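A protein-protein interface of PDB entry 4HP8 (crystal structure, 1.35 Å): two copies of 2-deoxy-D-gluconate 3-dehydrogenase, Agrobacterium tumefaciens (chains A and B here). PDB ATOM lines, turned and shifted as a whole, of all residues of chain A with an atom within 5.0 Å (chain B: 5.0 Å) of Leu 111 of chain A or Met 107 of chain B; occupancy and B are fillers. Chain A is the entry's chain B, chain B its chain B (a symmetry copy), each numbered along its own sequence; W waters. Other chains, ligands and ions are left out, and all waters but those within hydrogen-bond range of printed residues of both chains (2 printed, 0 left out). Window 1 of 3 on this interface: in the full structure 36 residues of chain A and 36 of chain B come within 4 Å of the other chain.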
ATOM      1  N   VAL A 106       4.201  -4.587  21.255  1.00  0.00           N
ATOM      2  CA  VAL A 106       4.863  -4.145  20.031  1.00  0.00           C
ATOM      3  C   VAL A 106       5.501  -5.323  19.288  1.00  0.00           C
ATOM      4  O   VAL A 106       5.348  -5.441  18.071  1.00  0.00           O
ATOM      5  CB  VAL A 106       5.916  -3.100  20.369  1.00  0.00           C
ATOM      6  CG1 VAL A 106       6.732  -2.715  19.124  1.00  0.00           C
ATOM      7  CG2 VAL A 106       5.208  -1.825  20.880  1.00  0.00           C
ATOM      8  N   MET A 107       6.169  -6.220  19.993  1.00  0.00           N
ATOM      9  CA  MET A 107       6.732  -7.382  19.324  1.00  0.00           C
ATOM     10  C   MET A 107       5.677  -8.248  18.701  1.00  0.00           C
ATOM     11  O   MET A 107       5.865  -8.798  17.608  1.00  0.00           O
ATOM     12  CB  MET A 107       7.553  -8.178  20.320  1.00  0.00           C
ATOM     13  CG  MET A 107       8.846  -7.507  20.579  1.00  0.00           C
ATOM     14  SD  MET A 107       9.946  -7.605  19.167  1.00  0.00           S
ATOM     15  CE  MET A 107      11.194  -6.449  19.678  1.00  0.00           C
ATOM     16  N   ASP A 108       4.568  -8.406  19.403  1.00  0.00           N
ATOM     17  CA  ASP A 108       3.510  -9.271  18.902  1.00  0.00           C
ATOM     18  C   ASP A 108       2.991  -8.762  17.549  1.00  0.00           C
ATOM     19  O   ASP A 108       2.844  -9.536  16.596  1.00  0.00           O
ATOM     20  CB  ASP A 108       2.331  -9.411  19.882  1.00  0.00           C
ATOM     21  CG  ASP A 108       2.556 -10.439  20.961  1.00  0.00           C
ATOM     22  OD1 ASP A 108       3.429 -11.319  20.803  1.00  0.00           O
ATOM     23  OD2 ASP A 108       1.799 -10.360  21.964  1.00  0.00           O
ATOM     24  N   VAL A 109       2.710  -7.470  17.436  1.00  0.00           N
ATOM     25  CA  VAL A 109       2.126  -6.985  16.192  1.00  0.00           C
ATOM     26  C   VAL A 109       3.207  -6.817  15.124  1.00  0.00           C
ATOM     27  O   VAL A 109       3.013  -7.199  13.972  1.00  0.00           O
ATOM     28  CB  VAL A 109       1.390  -5.660  16.399  1.00  0.00           C
ATOM     29  CG1 VAL A 109       0.901  -5.094  15.097  1.00  0.00           C
ATOM     30  CG2 VAL A 109       0.200  -5.849  17.384  1.00  0.00           C
ATOM     31  N   ASN A 110       4.323  -6.199  15.497  1.00  0.00           N
ATOM     32  CA  ASN A 110       5.276  -5.723  14.500  1.00  0.00           C
ATOM     33  C   ASN A 110       6.195  -6.798  14.001  1.00  0.00           C
ATOM     34  O   ASN A 110       6.731  -6.641  12.902  1.00  0.00           O
ATOM     35  CB  ASN A 110       6.160  -4.604  15.070  1.00  0.00           C
ATOM     36  CG  ASN A 110       5.387  -3.340  15.393  1.00  0.00           C
ATOM     37  OD1 ASN A 110       4.165  -3.324  15.556  1.00  0.00           O
ATOM     38  ND2 ASN A 110       6.139  -2.249  15.522  1.00  0.00           N
ATOM     39  N   LEU A 111       6.453  -7.836  14.782  1.00  0.00           N
ATOM     40  CA  LEU A 111       7.469  -8.815  14.415  1.00  0.00           C
ATOM     41  C   LEU A 111       6.912 -10.238  14.420  1.00  0.00           C
ATOM     42  O   LEU A 111       6.964 -10.927  13.383  1.00  0.00           O
ATOM     43  CB  LEU A 111       8.710  -8.697  15.322  1.00  0.00           C
ATOM     44  CG  LEU A 111       9.866  -9.587  14.901  1.00  0.00           C
ATOM     45  CD1 LEU A 111      10.427  -9.151  13.526  1.00  0.00           C
ATOM     46  CD2 LEU A 111      10.992  -9.588  15.939  1.00  0.00           C
ATOM     47  N   LYS A 112       6.371 -10.708  15.543  1.00  0.00           N
ATOM     48  CA  LYS A 112       5.855 -12.078  15.584  1.00  0.00           C
ATOM     49  C   LYS A 112       4.691 -12.283  14.617  1.00  0.00           C
ATOM     50  O   LYS A 112       4.665 -13.256  13.833  1.00  0.00           O
ATOM     51  CB  LYS A 112       5.478 -12.437  17.037  1.00  0.00           C
ATOM     52  CG  LYS A 112       5.071 -13.878  17.244  1.00  0.00           C
ATOM     53  CD  LYS A 112       4.911 -14.191  18.759  1.00  0.00           C
ATOM     54  CE  LYS A 112       4.375 -15.624  18.905  1.00  0.00           C
ATOM     55  NZ  LYS A 112       4.215 -15.987  20.349  1.00  0.00           N
ATOM     56  N   ALA A 113       3.703 -11.387  14.644  1.00  0.00           N
ATOM     57  CA  ALA A 113       2.580 -11.522  13.717  1.00  0.00           C
ATOM     58  C   ALA A 113       3.057 -11.393  12.287  1.00  0.00           C
ATOM     59  O   ALA A 113       2.512 -12.046  11.384  1.00  0.00           O
ATOM     60  CB  ALA A 113       1.496 -10.430  13.968  1.00  0.00           C
ATOM     61  N   LEU A 114       4.061 -10.541  12.031  1.00  0.00           N
ATOM     62  CA  LEU A 114       4.570 -10.387  10.667  1.00  0.00           C
ATOM     63  C   LEU A 114       5.158 -11.735  10.228  1.00  0.00           C
ATOM     64  O   LEU A 114       4.894 -12.198   9.103  1.00  0.00           O
ATOM     65  CB  LEU A 114       5.581  -9.227  10.599  1.00  0.00           C
ATOM     66  CG  LEU A 114       6.164  -8.950   9.231  1.00  0.00           C
ATOM     67  CD1 LEU A 114       6.426  -7.463   9.144  1.00  0.00           C
ATOM     68  CD2 LEU A 114       7.433  -9.709   8.930  1.00  0.00           C
ATOM     69  N   PHE A 115       5.944 -12.393  11.069  1.00  0.00           N
ATOM     70  CA  PHE A 115       6.513 -13.693  10.693  1.00  0.00           C
ATOM     71  C   PHE A 115       5.418 -14.728  10.466  1.00  0.00           C
ATOM     72  O   PHE A 115       5.406 -15.404   9.404  1.00  0.00           O
ATOM     73  CB  PHE A 115       7.481 -14.201  11.747  1.00  0.00           C
ATOM     74  CG  PHE A 115       7.981 -15.579  11.369  1.00  0.00           C
ATOM     75  CD1 PHE A 115       8.829 -15.742  10.289  1.00  0.00           C
ATOM     76  CD2 PHE A 115       7.495 -16.715  11.989  1.00  0.00           C
ATOM     77  CE1 PHE A 115       9.247 -17.026   9.852  1.00  0.00           C
ATOM     78  CE2 PHE A 115       7.888 -18.013  11.572  1.00  0.00           C
ATOM     79  CZ  PHE A 115       8.772 -18.159  10.494  1.00  0.00           C
ATOM     80  N   ALA A 154      13.879  -2.628  17.962  1.00  0.00           N
ATOM     81  CA  ALA A 154      14.242  -4.052  17.901  1.00  0.00           C
ATOM     82  C   ALA A 154      13.341  -4.777  16.921  1.00  0.00           C
ATOM     83  O   ALA A 154      13.864  -5.563  16.121  1.00  0.00           O
ATOM     84  CB  ALA A 154      14.164  -4.691  19.287  1.00  0.00           C
ATOM     85  N   ALA A 155      12.035  -4.525  16.928  1.00  0.00           N
ATOM     86  CA  ALA A 155      11.125  -5.196  16.039  1.00  0.00           C
ATOM     87  C   ALA A 155      11.428  -4.798  14.589  1.00  0.00           C
ATOM     88  O   ALA A 155      11.442  -5.684  13.700  1.00  0.00           O
ATOM     89  CB  ALA A 155       9.701  -4.820  16.377  1.00  0.00           C
ATOM     90  N   GLY A 158      14.356  -6.442  13.418  1.00  0.00           N
ATOM     91  CA  GLY A 158      13.949  -7.824  13.174  1.00  0.00           C
ATOM     92  C   GLY A 158      13.236  -7.998  11.847  1.00  0.00           C
ATOM     93  O   GLY A 158      13.432  -9.027  11.165  1.00  0.00           O
ATOM     94  N   VAL A 159      12.392  -7.056  11.438  1.00  0.00           N
ATOM     95  CA  VAL A 159      11.680  -7.139  10.163  1.00  0.00           C
ATOM     96  C   VAL A 159      12.674  -7.121   9.009  1.00  0.00           C
ATOM     97  O   VAL A 159      12.510  -7.895   8.048  1.00  0.00           O
ATOM     98  CB  VAL A 159      10.670  -5.986  10.031  1.00  0.00           C
ATOM     99  CG1 VAL A 159      10.079  -5.932   8.637  1.00  0.00           C
ATOM    100  CG2 VAL A 159       9.511  -6.166  11.044  1.00  0.00           C
ATOM    101  N   LEU A 162      14.180 -10.657   8.919  1.00  0.00           N
ATOM    102  CA  LEU A 162      13.304 -11.643   8.308  1.00  0.00           C
ATOM    103  C   LEU A 162      13.206 -11.432   6.826  1.00  0.00           C
ATOM    104  O   LEU A 162      13.069 -12.430   6.082  1.00  0.00           O
ATOM    105  CB  LEU A 162      11.888 -11.580   8.900  1.00  0.00           C
ATOM    106  CG  LEU A 162      11.780 -12.008  10.379  1.00  0.00           C
ATOM    107  CD1 LEU A 162      10.329 -11.750  10.839  1.00  0.00           C
ATOM    108  CD2 LEU A 162      12.168 -13.447  10.581  1.00  0.00           C
ATOM    109  N   TRP B 103      10.184 -20.003  17.966  1.00  0.00           N
ATOM    110  CA  TRP B 103      10.176 -18.561  17.924  1.00  0.00           C
ATOM    111  C   TRP B 103      10.354 -17.943  19.296  1.00  0.00           C
ATOM    112  O   TRP B 103      11.310 -17.192  19.553  1.00  0.00           O
ATOM    113  CB  TRP B 103       8.884 -18.082  17.251  1.00  0.00           C
ATOM    114  CG  TRP B 103       8.835 -16.563  17.220  1.00  0.00           C
ATOM    115  CD1 TRP B 103       8.366 -15.755  18.196  1.00  0.00           C
ATOM    116  CD2 TRP B 103       9.338 -15.689  16.186  1.00  0.00           C
ATOM    117  NE1 TRP B 103       8.533 -14.429  17.850  1.00  0.00           N
ATOM    118  CE2 TRP B 103       9.127 -14.375  16.606  1.00  0.00           C
ATOM    119  CE3 TRP B 103       9.913 -15.910  14.932  1.00  0.00           C
ATOM    120  CZ2 TRP B 103       9.502 -13.267  15.819  1.00  0.00           C
ATOM    121  CZ3 TRP B 103      10.335 -14.819  14.177  1.00  0.00           C
ATOM    122  CH2 TRP B 103      10.098 -13.508  14.612  1.00  0.00           C
ATOM    123  N   ASP B 104       9.440 -18.272  20.204  1.00  0.00           N
ATOM    124  CA  ASP B 104       9.393 -17.674  21.526  1.00  0.00           C
ATOM    125  C   ASP B 104      10.631 -17.951  22.359  1.00  0.00           C
ATOM    126  O   ASP B 104      11.168 -17.044  23.023  1.00  0.00           O
ATOM    127  CB  ASP B 104       8.181 -18.150  22.288  1.00  0.00           C
ATOM    128  CG  ASP B 104       6.877 -17.563  21.783  1.00  0.00           C
ATOM    129  OD1 ASP B 104       6.836 -16.500  21.134  1.00  0.00           O
ATOM    130  OD2 ASP B 104       5.831 -18.199  22.103  1.00  0.00           O
ATOM    131  N   GLU B 105      11.114 -19.195  22.357  1.00  0.00           N
ATOM    132  CA  GLU B 105      12.241 -19.503  23.265  1.00  0.00           C
ATOM    133  C   GLU B 105      13.531 -18.767  22.837  1.00  0.00           C
ATOM    134  O   GLU B 105      14.300 -18.281  23.679  1.00  0.00           O
ATOM    135  CB  GLU B 105      12.463 -20.991  23.401  1.00  0.00           C
ATOM    136  CG  GLU B 105      11.289 -21.642  24.141  1.00  0.00           C
ATOM    137  CD  GLU B 105      11.522 -23.080  24.524  1.00  0.00           C
ATOM    138  OE1 GLU B 105      12.216 -23.835  23.832  1.00  0.00           O
ATOM    139  OE2 GLU B 105      10.973 -23.467  25.588  1.00  0.00           O
ATOM    140  N   VAL B 106      13.756 -18.655  21.528  1.00  0.00           N
ATOM    141  CA  VAL B 106      14.900 -17.905  21.019  1.00  0.00           C
ATOM    142  C   VAL B 106      14.748 -16.406  21.295  1.00  0.00           C
ATOM    143  O   VAL B 106      15.696 -15.763  21.749  1.00  0.00           O
ATOM    144  CB  VAL B 106      15.049 -18.155  19.526  1.00  0.00           C
ATOM    145  CG1 VAL B 106      16.155 -17.271  18.926  1.00  0.00           C
ATOM    146  CG2 VAL B 106      15.455 -19.630  19.305  1.00  0.00           C
ATOM    147  N   MET B 107      13.569 -15.845  21.080  1.00  0.00           N
ATOM    148  CA  MET B 107      13.378 -14.439  21.392  1.00  0.00           C
ATOM    149  C   MET B 107      13.560 -14.149  22.852  1.00  0.00           C
ATOM    150  O   MET B 107      14.113 -13.109  23.234  1.00  0.00           O
ATOM    151  CB  MET B 107      11.996 -14.013  20.935  1.00  0.00           C
ATOM    152  CG  MET B 107      11.965 -13.850  19.464  1.00  0.00           C
ATOM    153  SD  MET B 107      12.893 -12.412  18.929  1.00  0.00           S
ATOM    154  CE  MET B 107      12.935 -12.717  17.180  1.00  0.00           C
ATOM    155  N   ASP B 108      13.069 -15.048  23.688  1.00  0.00           N
ATOM    156  CA  ASP B 108      13.152 -14.826  25.124  1.00  0.00           C
ATOM    157  C   ASP B 108      14.618 -14.710  25.568  1.00  0.00           C
ATOM    158  O   ASP B 108      14.983 -13.792  26.312  1.00  0.00           O
ATOM    159  CB  ASP B 108      12.455 -15.926  25.945  1.00  0.00           C
ATOM    160  CG  ASP B 108      10.966 -15.733  26.080  1.00  0.00           C
ATOM    161  OD1 ASP B 108      10.469 -14.604  25.876  1.00  0.00           O
ATOM    162  OD2 ASP B 108      10.309 -16.746  26.434  1.00  0.00           O
ATOM    163  N   VAL B 109      15.476 -15.620  25.126  1.00  0.00           N
ATOM    164  CA  VAL B 109      16.850 -15.585  25.612  1.00  0.00           C
ATOM    165  C   VAL B 109      17.650 -14.510  24.875  1.00  0.00           C
ATOM    166  O   VAL B 109      18.403 -13.759  25.490  1.00  0.00           O
ATOM    167  CB  VAL B 109      17.536 -16.942  25.454  1.00  0.00           C
ATOM    168  CG1 VAL B 109      18.987 -16.872  25.832  1.00  0.00           C
ATOM    169  CG2 VAL B 109      16.808 -18.020  26.311  1.00  0.00           C
ATOM    170  N   ASN B 110      17.523 -14.475  23.553  1.00  0.00           N
ATOM    171  CA  ASN B 110      18.457 -13.704  22.738  1.00  0.00           C
ATOM    172  C   ASN B 110      18.122 -12.244  22.677  1.00  0.00           C
ATOM    173  O   ASN B 110      19.022 -11.452  22.396  1.00  0.00           O
ATOM    174  CB  ASN B 110      18.485 -14.221  21.292  1.00  0.00           C
ATOM    175  CG  ASN B 110      19.048 -15.624  21.171  1.00  0.00           C
ATOM    176  OD1 ASN B 110      19.109 -16.407  22.122  1.00  0.00           O
ATOM    177  ND2 ASN B 110      19.440 -15.959  19.944  1.00  0.00           N
ATOM    178  N   LEU B 111      16.865 -11.866  22.854  1.00  0.00           N
ATOM    179  CA  LEU B 111      16.460 -10.483  22.633  1.00  0.00           C
ATOM    180  C   LEU B 111      15.744  -9.901  23.852  1.00  0.00           C
ATOM    181  O   LEU B 111      16.195  -8.880  24.406  1.00  0.00           O
ATOM    182  CB  LEU B 111      15.600 -10.349  21.362  1.00  0.00           C
ATOM    183  CG  LEU B 111      15.269  -8.914  20.991  1.00  0.00           C
ATOM    184  CD1 LEU B 111      16.547  -8.136  20.600  1.00  0.00           C
ATOM    185  CD2 LEU B 111      14.252  -8.841  19.848  1.00  0.00           C
ATOM    186  N   LYS B 112      14.648 -10.512  24.300  1.00  0.00           N
ATOM    187  CA  LYS B 112      13.926  -9.960  25.448  1.00  0.00           C
ATOM    188  C   LYS B 112      14.775  -9.963  26.717  1.00  0.00           C
ATOM    189  O   LYS B 112      14.873  -8.942  27.433  1.00  0.00           O
ATOM    190  CB  LYS B 112      12.598 -10.726  25.631  1.00  0.00           C
ATOM    191  CG  LYS B 112      11.684 -10.158  26.693  1.00  0.00           C
ATOM    192  CD  LYS B 112      10.300 -10.865  26.661  1.00  0.00           C
ATOM    193  CE  LYS B 112       9.460 -10.341  27.835  1.00  0.00           C
ATOM    194  NZ  LYS B 112       8.105 -10.979  27.846  1.00  0.00           N
ATOM    195  N   ALA B 113      15.406 -11.095  27.034  1.00  0.00           N
ATOM    196  CA  ALA B 113      16.255 -11.141  28.223  1.00  0.00           C
ATOM    197  C   ALA B 113      17.420 -10.185  28.077  1.00  0.00           C
ATOM    198  O   ALA B 113      17.872  -9.594  29.069  1.00  0.00           O
ATOM    199  CB  ALA B 113      16.827 -12.570  28.464  1.00  0.00           C
ATOM    200  N   SER B 151      13.831 -16.974  13.910  1.00  0.00           N
ATOM    201  CA  SER B 151      13.854 -16.268  15.188  1.00  0.00           C
ATOM    202  C   SER B 151      15.261 -15.828  15.574  1.00  0.00           C
ATOM    203  O   SER B 151      15.399 -14.755  16.195  1.00  0.00           O
ATOM    204  CB  SER B 151      13.157 -17.091  16.303  1.00  0.00           C
ATOM    205  OG  SER B 151      13.803 -18.371  16.452  1.00  0.00           O
ATOM    206  N   ALA B 154      16.066 -12.697  13.312  1.00  0.00           N
ATOM    207  CA  ALA B 154      15.263 -11.564  13.796  1.00  0.00           C
ATOM    208  C   ALA B 154      15.791 -11.085  15.133  1.00  0.00           C
ATOM    209  O   ALA B 154      15.923  -9.866  15.305  1.00  0.00           O
ATOM    210  CB  ALA B 154      13.788 -11.951  13.901  1.00  0.00           C
ATOM    211  N   ALA B 155      16.125 -11.979  16.060  1.00  0.00           N
ATOM    212  CA  ALA B 155      16.611 -11.587  17.356  1.00  0.00           C
ATOM    213  C   ALA B 155      17.969 -10.889  17.212  1.00  0.00           C
ATOM    214  O   ALA B 155      18.194  -9.844  17.870  1.00  0.00           O
ATOM    215  CB  ALA B 155      16.763 -12.804  18.239  1.00  0.00           C
HETATM  216  O   HOH W   1      10.363 -10.707  20.062  1.00  0.00           O
HETATM  217  O   HOH W   2       3.760 -17.114  23.421  1.00  0.00           O
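Of the printed residues of chain B, Leu 111 of chain A touches Trp 103 and Met 107.
Of the printed residues of chain A, Met 107 of chain B touches Leu 111.
Printed residues of chain B within 4 Å of Phe 115 of chain A: Trp 103 (3.7 Å).
Printed residues of chain A within 4 Å of Ala 154 of chain B: Gly 158 and Leu 162.
Printed residues of chain B within 4 Å of Leu 162 of chain A: Ala 154.
Of the printed residues of chain A, Asp 104 of chain B touches Lys 112.
Asn 110 of chain A touches none of the printed residues of chain B.
Met 107 of chain A touches Leu 111 of chain B (CE to CD2, 3.9 Å).
Trp 103 of chain B touches Leu 111 of chain A.
Met 107 of chain B touches Leu 111 of chain A.
Trp 103 of chain B touches Lys 112 of chain A (NE1 to CG, 3.6 Å).
Trp 103 of chain B touches Phe 115 of chain A.
Gly 158 of chain A touches Ala 154 of chain B.
Leu 162 of chain A touches Ala 154 of chain B (CD2 to CB, 3.99 Å).
Water W2 lies within hydrogen-bond range of OD2 of Asp 104 of chain B and NZ of Lys 112 of chain A.
Water W1 lies within hydrogen-bond range of the side-chain sulfur (SD) of Met 107 of chain A (3.3 Å) and the side-chain sulfur (SD) of Met 107 of chain B (3.3 Å).
Hydrophobic or aromatic side chains of chain B within 4 Å of the printed part of chain A: Trp 103, Met 107, Leu 111 and Ala 154.
Printed residues of chain A that touch a printed residue of chain B: Met 107, Leu 111, Lys 112, Phe 115, Gly 158 and Leu 162.
The backbone carbonyl oxygen of Met 107 of chain A is in hydrogen-bond range of the backbone NH of Lys 112 of chain A.
N of Lys 112 of chain B sits at hydrogen-bond distance from O of Met 107 of chain B (2.9 Å).
The side-chain carboxylate (OD1) of Asp 104 of chain B is in salt-bridge range of the side-chain amino group (NZ) of Lys 112 of chain A, at 2.8 Å.
Met 107 of chain A touches Leu 111 of chain B, and with the chains exchanged Leu 111 of chain A touches Met 107 of chain B.
Positions printed for both chains: 106, 107, 108, 109, 110, 111, 112, 113, 154 and 155.
Of the 8 pairs that touch across the chains among the printed residues, 2 have their exchanged pair printed and touching as well.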
